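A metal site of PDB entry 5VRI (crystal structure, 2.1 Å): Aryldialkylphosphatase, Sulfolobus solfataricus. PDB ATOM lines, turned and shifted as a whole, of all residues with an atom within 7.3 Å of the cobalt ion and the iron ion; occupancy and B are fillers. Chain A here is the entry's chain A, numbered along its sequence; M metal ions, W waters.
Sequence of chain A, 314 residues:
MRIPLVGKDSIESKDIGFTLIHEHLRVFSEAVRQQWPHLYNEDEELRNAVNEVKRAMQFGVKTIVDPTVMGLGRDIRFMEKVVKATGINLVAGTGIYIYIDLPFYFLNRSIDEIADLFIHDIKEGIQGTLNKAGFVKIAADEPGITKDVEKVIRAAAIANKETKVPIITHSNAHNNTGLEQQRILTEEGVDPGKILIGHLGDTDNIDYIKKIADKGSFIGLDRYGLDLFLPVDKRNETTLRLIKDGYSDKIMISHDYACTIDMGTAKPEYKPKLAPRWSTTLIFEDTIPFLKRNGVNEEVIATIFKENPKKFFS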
ATOM      1  N   HIS A  22      27.786  15.826  31.529  1.00  0.00           N
ATOM      2  CA  HIS A  22      26.827  16.767  30.924  1.00  0.00           C
ATOM      3  C   HIS A  22      25.495  16.079  30.600  1.00  0.00           C
ATOM      4  O   HIS A  22      25.325  15.518  29.507  1.00  0.00           O
ATOM      5  CB  HIS A  22      27.414  17.414  29.656  1.00  0.00           C
ATOM      6  CG  HIS A  22      26.624  18.571  29.128  1.00  0.00           C
ATOM      7  ND1 HIS A  22      27.200  19.781  28.786  1.00  0.00           N
ATOM      8  CD2 HIS A  22      25.297  18.708  28.857  1.00  0.00           C
ATOM      9  CE1 HIS A  22      26.268  20.608  28.343  1.00  0.00           C
ATOM     10  NE2 HIS A  22      25.100  19.976  28.367  1.00  0.00           N
ATOM     11  N   GLU A  23      24.561  16.127  31.543  1.00  0.00           N
ATOM     12  CA  GLU A  23      23.208  15.617  31.328  1.00  0.00           C
ATOM     13  C   GLU A  23      22.209  16.569  31.994  1.00  0.00           C
ATOM     14  O   GLU A  23      22.503  17.142  33.050  1.00  0.00           O
ATOM     15  CB  GLU A  23      23.050  14.208  31.892  1.00  0.00           C
ATOM     16  CG  GLU A  23      24.179  13.242  31.520  1.00  0.00           C
ATOM     17  CD  GLU A  23      24.106  12.775  30.075  1.00  0.00           C
ATOM     18  OE1 GLU A  23      25.105  12.213  29.590  1.00  0.00           O
ATOM     19  OE2 GLU A  23      23.052  12.966  29.428  1.00  0.00           O
ATOM     20  N   HIS A  24      21.037  16.718  31.376  1.00  0.00           N
ATOM     21  CA  HIS A  24      20.005  17.632  31.889  1.00  0.00           C
ATOM     22  C   HIS A  24      18.797  16.843  32.422  1.00  0.00           C
ATOM     23  O   HIS A  24      18.267  15.972  31.735  1.00  0.00           O
ATOM     24  CB  HIS A  24      19.539  18.609  30.790  1.00  0.00           C
ATOM     25  CG  HIS A  24      20.638  19.423  30.166  1.00  0.00           C
ATOM     26  ND1 HIS A  24      20.996  20.669  30.626  1.00  0.00           N
ATOM     27  CD2 HIS A  24      21.420  19.200  29.078  1.00  0.00           C
ATOM     28  CE1 HIS A  24      21.964  21.170  29.879  1.00  0.00           C
ATOM     29  NE2 HIS A  24      22.240  20.295  28.920  1.00  0.00           N
ATOM     30  N   VAL A  27      14.745  20.713  30.863  1.00  0.00           N
ATOM     31  CA  VAL A  27      15.044  21.992  30.221  1.00  0.00           C
ATOM     32  C   VAL A  27      13.754  22.694  29.784  1.00  0.00           C
ATOM     33  O   VAL A  27      12.839  22.061  29.260  1.00  0.00           O
ATOM     34  CB  VAL A  27      15.959  21.803  28.995  1.00  0.00           C
ATOM     35  CG1 VAL A  27      16.058  23.095  28.193  1.00  0.00           C
ATOM     36  CG2 VAL A  27      17.342  21.338  29.442  1.00  0.00           C
ATOM     37  N   ASP A  66      24.773  18.387  36.080  1.00  0.00           N
ATOM     38  CA  ASP A  66      23.672  18.961  35.309  1.00  0.00           C
ATOM     39  C   ASP A  66      23.871  20.459  35.090  1.00  0.00           C
ATOM     40  O   ASP A  66      23.658  21.252  36.005  1.00  0.00           O
ATOM     41  CB  ASP A  66      22.340  18.712  36.041  1.00  0.00           C
ATOM     42  CG  ASP A  66      21.134  19.189  35.249  1.00  0.00           C
ATOM     43  OD1 ASP A  66      21.312  20.074  34.384  1.00  0.00           O
ATOM     44  OD2 ASP A  66      20.026  18.696  35.511  1.00  0.00           O
ATOM     45  N   PRO A  67      24.290  20.828  33.866  1.00  0.00           N
ATOM     46  CA  PRO A  67      24.598  22.220  33.527  1.00  0.00           C
ATOM     47  C   PRO A  67      23.367  23.052  33.146  1.00  0.00           C
ATOM     48  O   PRO A  67      23.477  23.982  32.345  1.00  0.00           O
ATOM     49  CB  PRO A  67      25.540  22.082  32.324  1.00  0.00           C
ATOM     50  CG  PRO A  67      25.169  20.786  31.702  1.00  0.00           C
ATOM     51  CD  PRO A  67      24.541  19.906  32.744  1.00  0.00           C
ATOM     52  N   THR A  68      22.206  22.718  33.704  1.00  0.00           N
ATOM     53  CA  THR A  68      21.009  23.521  33.497  1.00  0.00           C
ATOM     54  C   THR A  68      21.108  24.788  34.343  1.00  0.00           C
ATOM     55  O   THR A  68      21.093  24.721  35.577  1.00  0.00           O
ATOM     56  CB  THR A  68      19.729  22.740  33.881  1.00  0.00           C
ATOM     57  OG1 THR A  68      19.724  21.456  33.235  1.00  0.00           O
ATOM     58  CG2 THR A  68      18.474  23.521  33.457  1.00  0.00           C
ATOM     59  N   LEU A  72      17.986  27.966  30.614  1.00  0.00           N
ATOM     60  CA  LEU A  72      17.629  26.560  30.375  1.00  0.00           C
ATOM     61  C   LEU A  72      16.606  26.065  31.398  1.00  0.00           C
ATOM     62  O   LEU A  72      16.201  24.908  31.356  1.00  0.00           O
ATOM     63  CB  LEU A  72      18.879  25.674  30.406  1.00  0.00           C
ATOM     64  CG  LEU A  72      19.904  25.877  29.302  1.00  0.00           C
ATOM     65  CD1 LEU A  72      21.085  24.939  29.517  1.00  0.00           C
ATOM     66  CD2 LEU A  72      19.291  25.670  27.925  1.00  0.00           C
ATOM     67  N   TYR A  97      23.180  31.133  30.158  1.00  0.00           N
ATOM     68  CA  TYR A  97      23.182  30.474  28.851  1.00  0.00           C
ATOM     69  C   TYR A  97      22.513  31.385  27.832  1.00  0.00           C
ATOM     70  O   TYR A  97      21.284  31.475  27.781  1.00  0.00           O
ATOM     71  CB  TYR A  97      22.446  29.137  28.976  1.00  0.00           C
ATOM     72  CG  TYR A  97      22.399  28.269  27.734  1.00  0.00           C
ATOM     73  CD1 TYR A  97      21.522  28.564  26.693  1.00  0.00           C
ATOM     74  CD2 TYR A  97      23.193  27.137  27.619  1.00  0.00           C
ATOM     75  CE1 TYR A  97      21.469  27.768  25.561  1.00  0.00           C
ATOM     76  CE2 TYR A  97      23.145  26.332  26.488  1.00  0.00           C
ATOM     77  CZ  TYR A  97      22.272  26.654  25.468  1.00  0.00           C
ATOM     78  OH  TYR A  97      22.205  25.862  24.344  1.00  0.00           O
ATOM     79  N   TYR A  99      22.878  33.101  23.540  1.00  0.00           N
ATOM     80  CA  TYR A  99      23.509  33.021  22.215  1.00  0.00           C
ATOM     81  C   TYR A  99      23.829  34.408  21.657  1.00  0.00           C
ATOM     82  O   TYR A  99      24.742  34.552  20.853  1.00  0.00           O
ATOM     83  CB  TYR A  99      22.595  32.283  21.239  1.00  0.00           C
ATOM     84  CG  TYR A  99      22.529  30.779  21.431  1.00  0.00           C
ATOM     85  CD1 TYR A  99      22.975  30.187  22.599  1.00  0.00           C
ATOM     86  CD2 TYR A  99      21.996  29.969  20.432  1.00  0.00           C
ATOM     87  CE1 TYR A  99      22.899  28.803  22.770  1.00  0.00           C
ATOM     88  CE2 TYR A  99      21.911  28.603  20.592  1.00  0.00           C
ATOM     89  CZ  TYR A  99      22.361  28.024  21.761  1.00  0.00           C
ATOM     90  OH  TYR A  99      22.277  26.658  21.911  1.00  0.00           O
ATOM     91  N   KCX A 137      28.532  27.567  34.227  1.00  0.00           N
ATOM     92  CA  KCX A 137      28.247  27.178  32.842  1.00  0.00           C
ATOM     93  CB  KCX A 137      27.012  26.273  32.799  1.00  0.00           C
ATOM     94  CG  KCX A 137      26.380  26.181  31.410  1.00  0.00           C
ATOM     95  CD  KCX A 137      27.047  25.119  30.539  1.00  0.00           C
ATOM     96  CE  KCX A 137      26.393  25.004  29.158  1.00  0.00           C
ATOM     97  NZ  KCX A 137      25.251  24.109  29.174  1.00  0.00           N
ATOM     98  C   KCX A 137      27.995  28.419  32.015  1.00  0.00           C
ATOM     99  O   KCX A 137      27.245  29.304  32.425  1.00  0.00           O
ATOM    100  CX  KCX A 137      24.843  23.347  28.157  1.00  0.00           C
ATOM    101  OQ1 KCX A 137      23.873  22.637  28.281  1.00  0.00           O
ATOM    102  OQ2 KCX A 137      25.460  23.347  26.962  1.00  0.00           O
ATOM    103  N   ILE A 138      28.640  28.483  30.863  1.00  0.00           N
ATOM    104  CA  ILE A 138      28.443  29.588  29.931  1.00  0.00           C
ATOM    105  C   ILE A 138      28.286  29.041  28.518  1.00  0.00           C
ATOM    106  O   ILE A 138      28.555  27.855  28.281  1.00  0.00           O
ATOM    107  CB  ILE A 138      29.610  30.606  29.998  1.00  0.00           C
ATOM    108  CG1 ILE A 138      30.948  29.926  29.707  1.00  0.00           C
ATOM    109  CG2 ILE A 138      29.647  31.268  31.370  1.00  0.00           C
ATOM    110  CD1 ILE A 138      31.264  29.795  28.231  1.00  0.00           C
ATOM    111  N   ALA A 139      27.831  29.871  27.580  1.00  0.00           N
ATOM    112  CA  ALA A 139      27.541  29.378  26.245  1.00  0.00           C
ATOM    113  C   ALA A 139      27.898  30.340  25.116  1.00  0.00           C
ATOM    114  O   ALA A 139      27.992  31.547  25.318  1.00  0.00           O
ATOM    115  CB  ALA A 139      26.080  28.975  26.150  1.00  0.00           C
ATOM    116  N   ASP A 141      27.231  30.086  20.497  1.00  0.00           N
ATOM    117  CA  ASP A 141      26.842  29.226  19.392  1.00  0.00           C
ATOM    118  C   ASP A 141      27.076  29.897  18.040  1.00  0.00           C
ATOM    119  O   ASP A 141      28.088  30.569  17.830  1.00  0.00           O
ATOM    120  CB  ASP A 141      25.381  28.778  19.539  1.00  0.00           C
ATOM    121  CG  ASP A 141      25.111  27.434  18.876  1.00  0.00           C
ATOM    122  OD1 ASP A 141      24.976  27.381  17.637  1.00  0.00           O
ATOM    123  OD2 ASP A 141      25.028  26.411  19.600  1.00  0.00           O
ATOM    124  N   THR A 169      31.472  24.682  29.378  1.00  0.00           N
ATOM    125  CA  THR A 169      30.978  25.541  28.315  1.00  0.00           C
ATOM    126  C   THR A 169      30.110  24.814  27.284  1.00  0.00           C
ATOM    127  O   THR A 169      30.169  23.594  27.137  1.00  0.00           O
ATOM    128  CB  THR A 169      32.095  26.288  27.553  1.00  0.00           C
ATOM    129  OG1 THR A 169      32.504  25.515  26.416  1.00  0.00           O
ATOM    130  CG2 THR A 169      33.288  26.572  28.475  1.00  0.00           C
ATOM    131  N   HIS A 170      29.318  25.603  26.584  1.00  0.00           N
ATOM    132  CA  HIS A 170      28.557  25.151  25.443  1.00  0.00           C
ATOM    133  C   HIS A 170      29.117  25.914  24.243  1.00  0.00           C
ATOM    134  O   HIS A 170      29.244  27.131  24.288  1.00  0.00           O
ATOM    135  CB  HIS A 170      27.080  25.505  25.649  1.00  0.00           C
ATOM    136  CG  HIS A 170      26.221  25.294  24.448  1.00  0.00           C
ATOM    137  ND1 HIS A 170      25.309  24.259  24.356  1.00  0.00           N
ATOM    138  CD2 HIS A 170      26.124  25.983  23.285  1.00  0.00           C
ATOM    139  CE1 HIS A 170      24.691  24.326  23.190  1.00  0.00           C
ATOM    140  NE2 HIS A 170      25.170  25.360  22.516  1.00  0.00           N
ATOM    141  N   SER A 171      29.488  25.192  23.193  1.00  0.00           N
ATOM    142  CA  SER A 171      29.982  25.848  21.997  1.00  0.00           C
ATOM    143  C   SER A 171      29.459  25.190  20.719  1.00  0.00           C
ATOM    144  O   SER A 171      28.855  24.120  20.767  1.00  0.00           O
ATOM    145  CB  SER A 171      31.516  25.906  21.978  1.00  0.00           C
ATOM    146  OG  SER A 171      32.068  24.687  21.538  1.00  0.00           O
ATOM    147  N   GLY A 198      32.748  22.493  25.560  1.00  0.00           N
ATOM    148  CA  GLY A 198      31.656  21.564  25.270  1.00  0.00           C
ATOM    149  C   GLY A 198      31.280  21.384  23.816  1.00  0.00           C
ATOM    150  O   GLY A 198      31.532  22.255  22.978  1.00  0.00           O
ATOM    151  N   HIS A 199      30.686  20.233  23.534  1.00  0.00           N
ATOM    152  CA  HIS A 199      30.046  19.958  22.244  1.00  0.00           C
ATOM    153  C   HIS A 199      31.057  19.792  21.088  1.00  0.00           C
ATOM    154  O   HIS A 199      30.708  19.897  19.918  1.00  0.00           O
ATOM    155  CB  HIS A 199      28.949  21.008  21.927  1.00  0.00           C
ATOM    156  CG  HIS A 199      27.941  21.195  23.043  1.00  0.00           C
ATOM    157  ND1 HIS A 199      27.643  20.210  23.957  1.00  0.00           N
ATOM    158  CD2 HIS A 199      27.143  22.243  23.348  1.00  0.00           C
ATOM    159  CE1 HIS A 199      26.723  20.652  24.801  1.00  0.00           C
ATOM    160  NE2 HIS A 199      26.401  21.891  24.460  1.00  0.00           N
ATOM    161  N   ASP A 222      30.402  15.080  24.039  1.00  0.00           N
ATOM    162  CA  ASP A 222      29.371  15.042  25.062  1.00  0.00           C
ATOM    163  C   ASP A 222      27.924  15.005  24.567  1.00  0.00           C
ATOM    164  O   ASP A 222      26.997  15.209  25.350  1.00  0.00           O
ATOM    165  CB  ASP A 222      29.559  16.239  26.007  1.00  0.00           C
ATOM    166  CG  ASP A 222      29.618  17.570  25.262  1.00  0.00           C
ATOM    167  OD1 ASP A 222      29.181  17.625  24.094  1.00  0.00           O
ATOM    168  OD2 ASP A 222      30.116  18.555  25.836  1.00  0.00           O
ATOM    169  N   ARG A 223      27.725  14.729  23.281  1.00  0.00           N
ATOM    170  CA  ARG A 223      26.363  14.692  22.735  1.00  0.00           C
ATOM    171  C   ARG A 223      26.037  13.371  22.037  1.00  0.00           C
ATOM    172  O   ARG A 223      25.303  13.347  21.050  1.00  0.00           O
ATOM    173  CB  ARG A 223      26.136  15.871  21.780  1.00  0.00           C
ATOM    174  CG  ARG A 223      25.698  17.148  22.493  1.00  0.00           C
ATOM    175  CD  ARG A 223      25.658  18.342  21.556  1.00  0.00           C
ATOM    176  NE  ARG A 223      24.765  19.381  22.053  1.00  0.00           N
ATOM    177  CZ  ARG A 223      24.608  20.574  21.477  1.00  0.00           C
ATOM    178  NH1 ARG A 223      23.758  21.454  21.997  1.00  0.00           N
ATOM    179  NH2 ARG A 223      25.300  20.888  20.390  1.00  0.00           N
ATOM    180  N   HIS A 255      26.077  12.564  27.114  1.00  0.00           N
ATOM    181  CA  HIS A 255      24.993  12.524  26.132  1.00  0.00           C
ATOM    182  C   HIS A 255      24.287  13.862  25.924  1.00  0.00           C
ATOM    183  O   HIS A 255      23.615  14.057  24.904  1.00  0.00           O
ATOM    184  CB  HIS A 255      23.944  11.484  26.519  1.00  0.00           C
ATOM    185  CG  HIS A 255      24.497  10.133  26.822  1.00  0.00           C
ATOM    186  ND1 HIS A 255      24.888   9.758  28.096  1.00  0.00           N
ATOM    187  CD2 HIS A 255      24.724   9.055  26.029  1.00  0.00           C
ATOM    188  CE1 HIS A 255      25.325   8.506  28.067  1.00  0.00           C
ATOM    189  NE2 HIS A 255      25.239   8.066  26.832  1.00  0.00           N
ATOM    190  N   ASP A 256      24.404  14.778  26.882  1.00  0.00           N
ATOM    191  CA  ASP A 256      23.632  16.018  26.848  1.00  0.00           C
ATOM    192  C   ASP A 256      22.146  15.681  26.741  1.00  0.00           C
ATOM    193  O   ASP A 256      21.372  16.390  26.083  1.00  0.00           O
ATOM    194  CB  ASP A 256      24.077  16.913  25.688  1.00  0.00           C
ATOM    195  CG  ASP A 256      23.597  18.364  25.814  1.00  0.00           C
ATOM    196  OD1 ASP A 256      23.270  18.815  26.938  1.00  0.00           O
ATOM    197  OD2 ASP A 256      23.578  19.058  24.779  1.00  0.00           O
ATOM    198  N   TYR A 257      21.742  14.584  27.372  1.00  0.00           N
ATOM    199  CA  TYR A 257      20.344  14.176  27.364  1.00  0.00           C
ATOM    200  C   TYR A 257      19.492  15.151  28.166  1.00  0.00           C
ATOM    201  O   TYR A 257      19.946  15.741  29.147  1.00  0.00           O
ATOM    202  CB  TYR A 257      20.184  12.753  27.919  1.00  0.00           C
ATOM    203  CG  TYR A 257      18.796  12.188  27.680  1.00  0.00           C
ATOM    204  CD1 TYR A 257      18.335  11.923  26.398  1.00  0.00           C
ATOM    205  CD2 TYR A 257      17.930  11.935  28.749  1.00  0.00           C
ATOM    206  CE1 TYR A 257      17.072  11.419  26.172  1.00  0.00           C
ATOM    207  CE2 TYR A 257      16.667  11.431  28.533  1.00  0.00           C
ATOM    208  CZ  TYR A 257      16.238  11.173  27.244  1.00  0.00           C
ATOM    209  OH  TYR A 257      14.985  10.673  27.009  1.00  0.00           O
HETATM  210 CO    CO M   1      25.068  22.758  25.365  1.00  0.00          CO
HETATM  211 FE    FE M   2      23.543  20.729  27.642  1.00  0.00          FE
HETATM  212  O   HOH W   1      23.872  21.579  25.817  1.00  0.00           O
HETATM  213  O   HOH W   2      21.737  22.942  24.795  1.00  0.00           O
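N of His 170 is in hydrogen-bond range of O of Ile 138, 2.9 Å away.
The side-chain carboxylate of Asp 256 lies within salt-bridge range of the guanidinium group of Arg 223.
A ring nitrogen (ND1) of His 170 sits close to the side-chain hydroxyl (OH) of Tyr 97 (3.5 Å).
O of Asp 222 lies within hydrogen-bond range of N of Asp 256, at 3.0 Å.
N of His 24 is in hydrogen-bond range of O of Tyr 257.
A ring nitrogen (ND1) of His 24 is in hydrogen-bond range of the side-chain hydroxyl (OG1) of Thr 68 (3.0 Å).
A ring nitrogen (NE2) of His 170 sits at hydrogen-bond distance from the side-chain carboxylate (OD2) of Asp 141.
OE2 of Glu 23 is in hydrogen-bond range of N of Asp 256 (3.4 Å).
The iron ion is bound by a ring nitrogen (NE2) of His 24 (1.9 Å).
NE2 of His 22 is bound to the iron ion (1.9 Å).
The iron ion is bound by OQ1 of KCX 137 (2.0 Å).
The iron ion is bound by water W1, 2.0 Å away.
The iron ion is bound by OD1 of Asp 256 (2.1 Å).
The iron ion has five donor atoms within binding distance.
NH1 of Arg 223 touches the cobalt ion, at 3.8 Å.
The nearest printed residue that does not touch the cobalt ion is Asp 256 (4.03 Å).
Of the 24 residues printed, 4 come within 4 Å of the iron ion.
The nearest printed residue that does not touch the iron ion is His 199 (4.3 Å).
The cobalt ion is bound by water W1 (1.7 Å), OQ2 of KCX 137 (1.7 Å), ND1 of His 170 (1.8 Å) and NE2 of His 199 (1.8 Å).
The cobalt ion has four donor atoms within binding distance.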
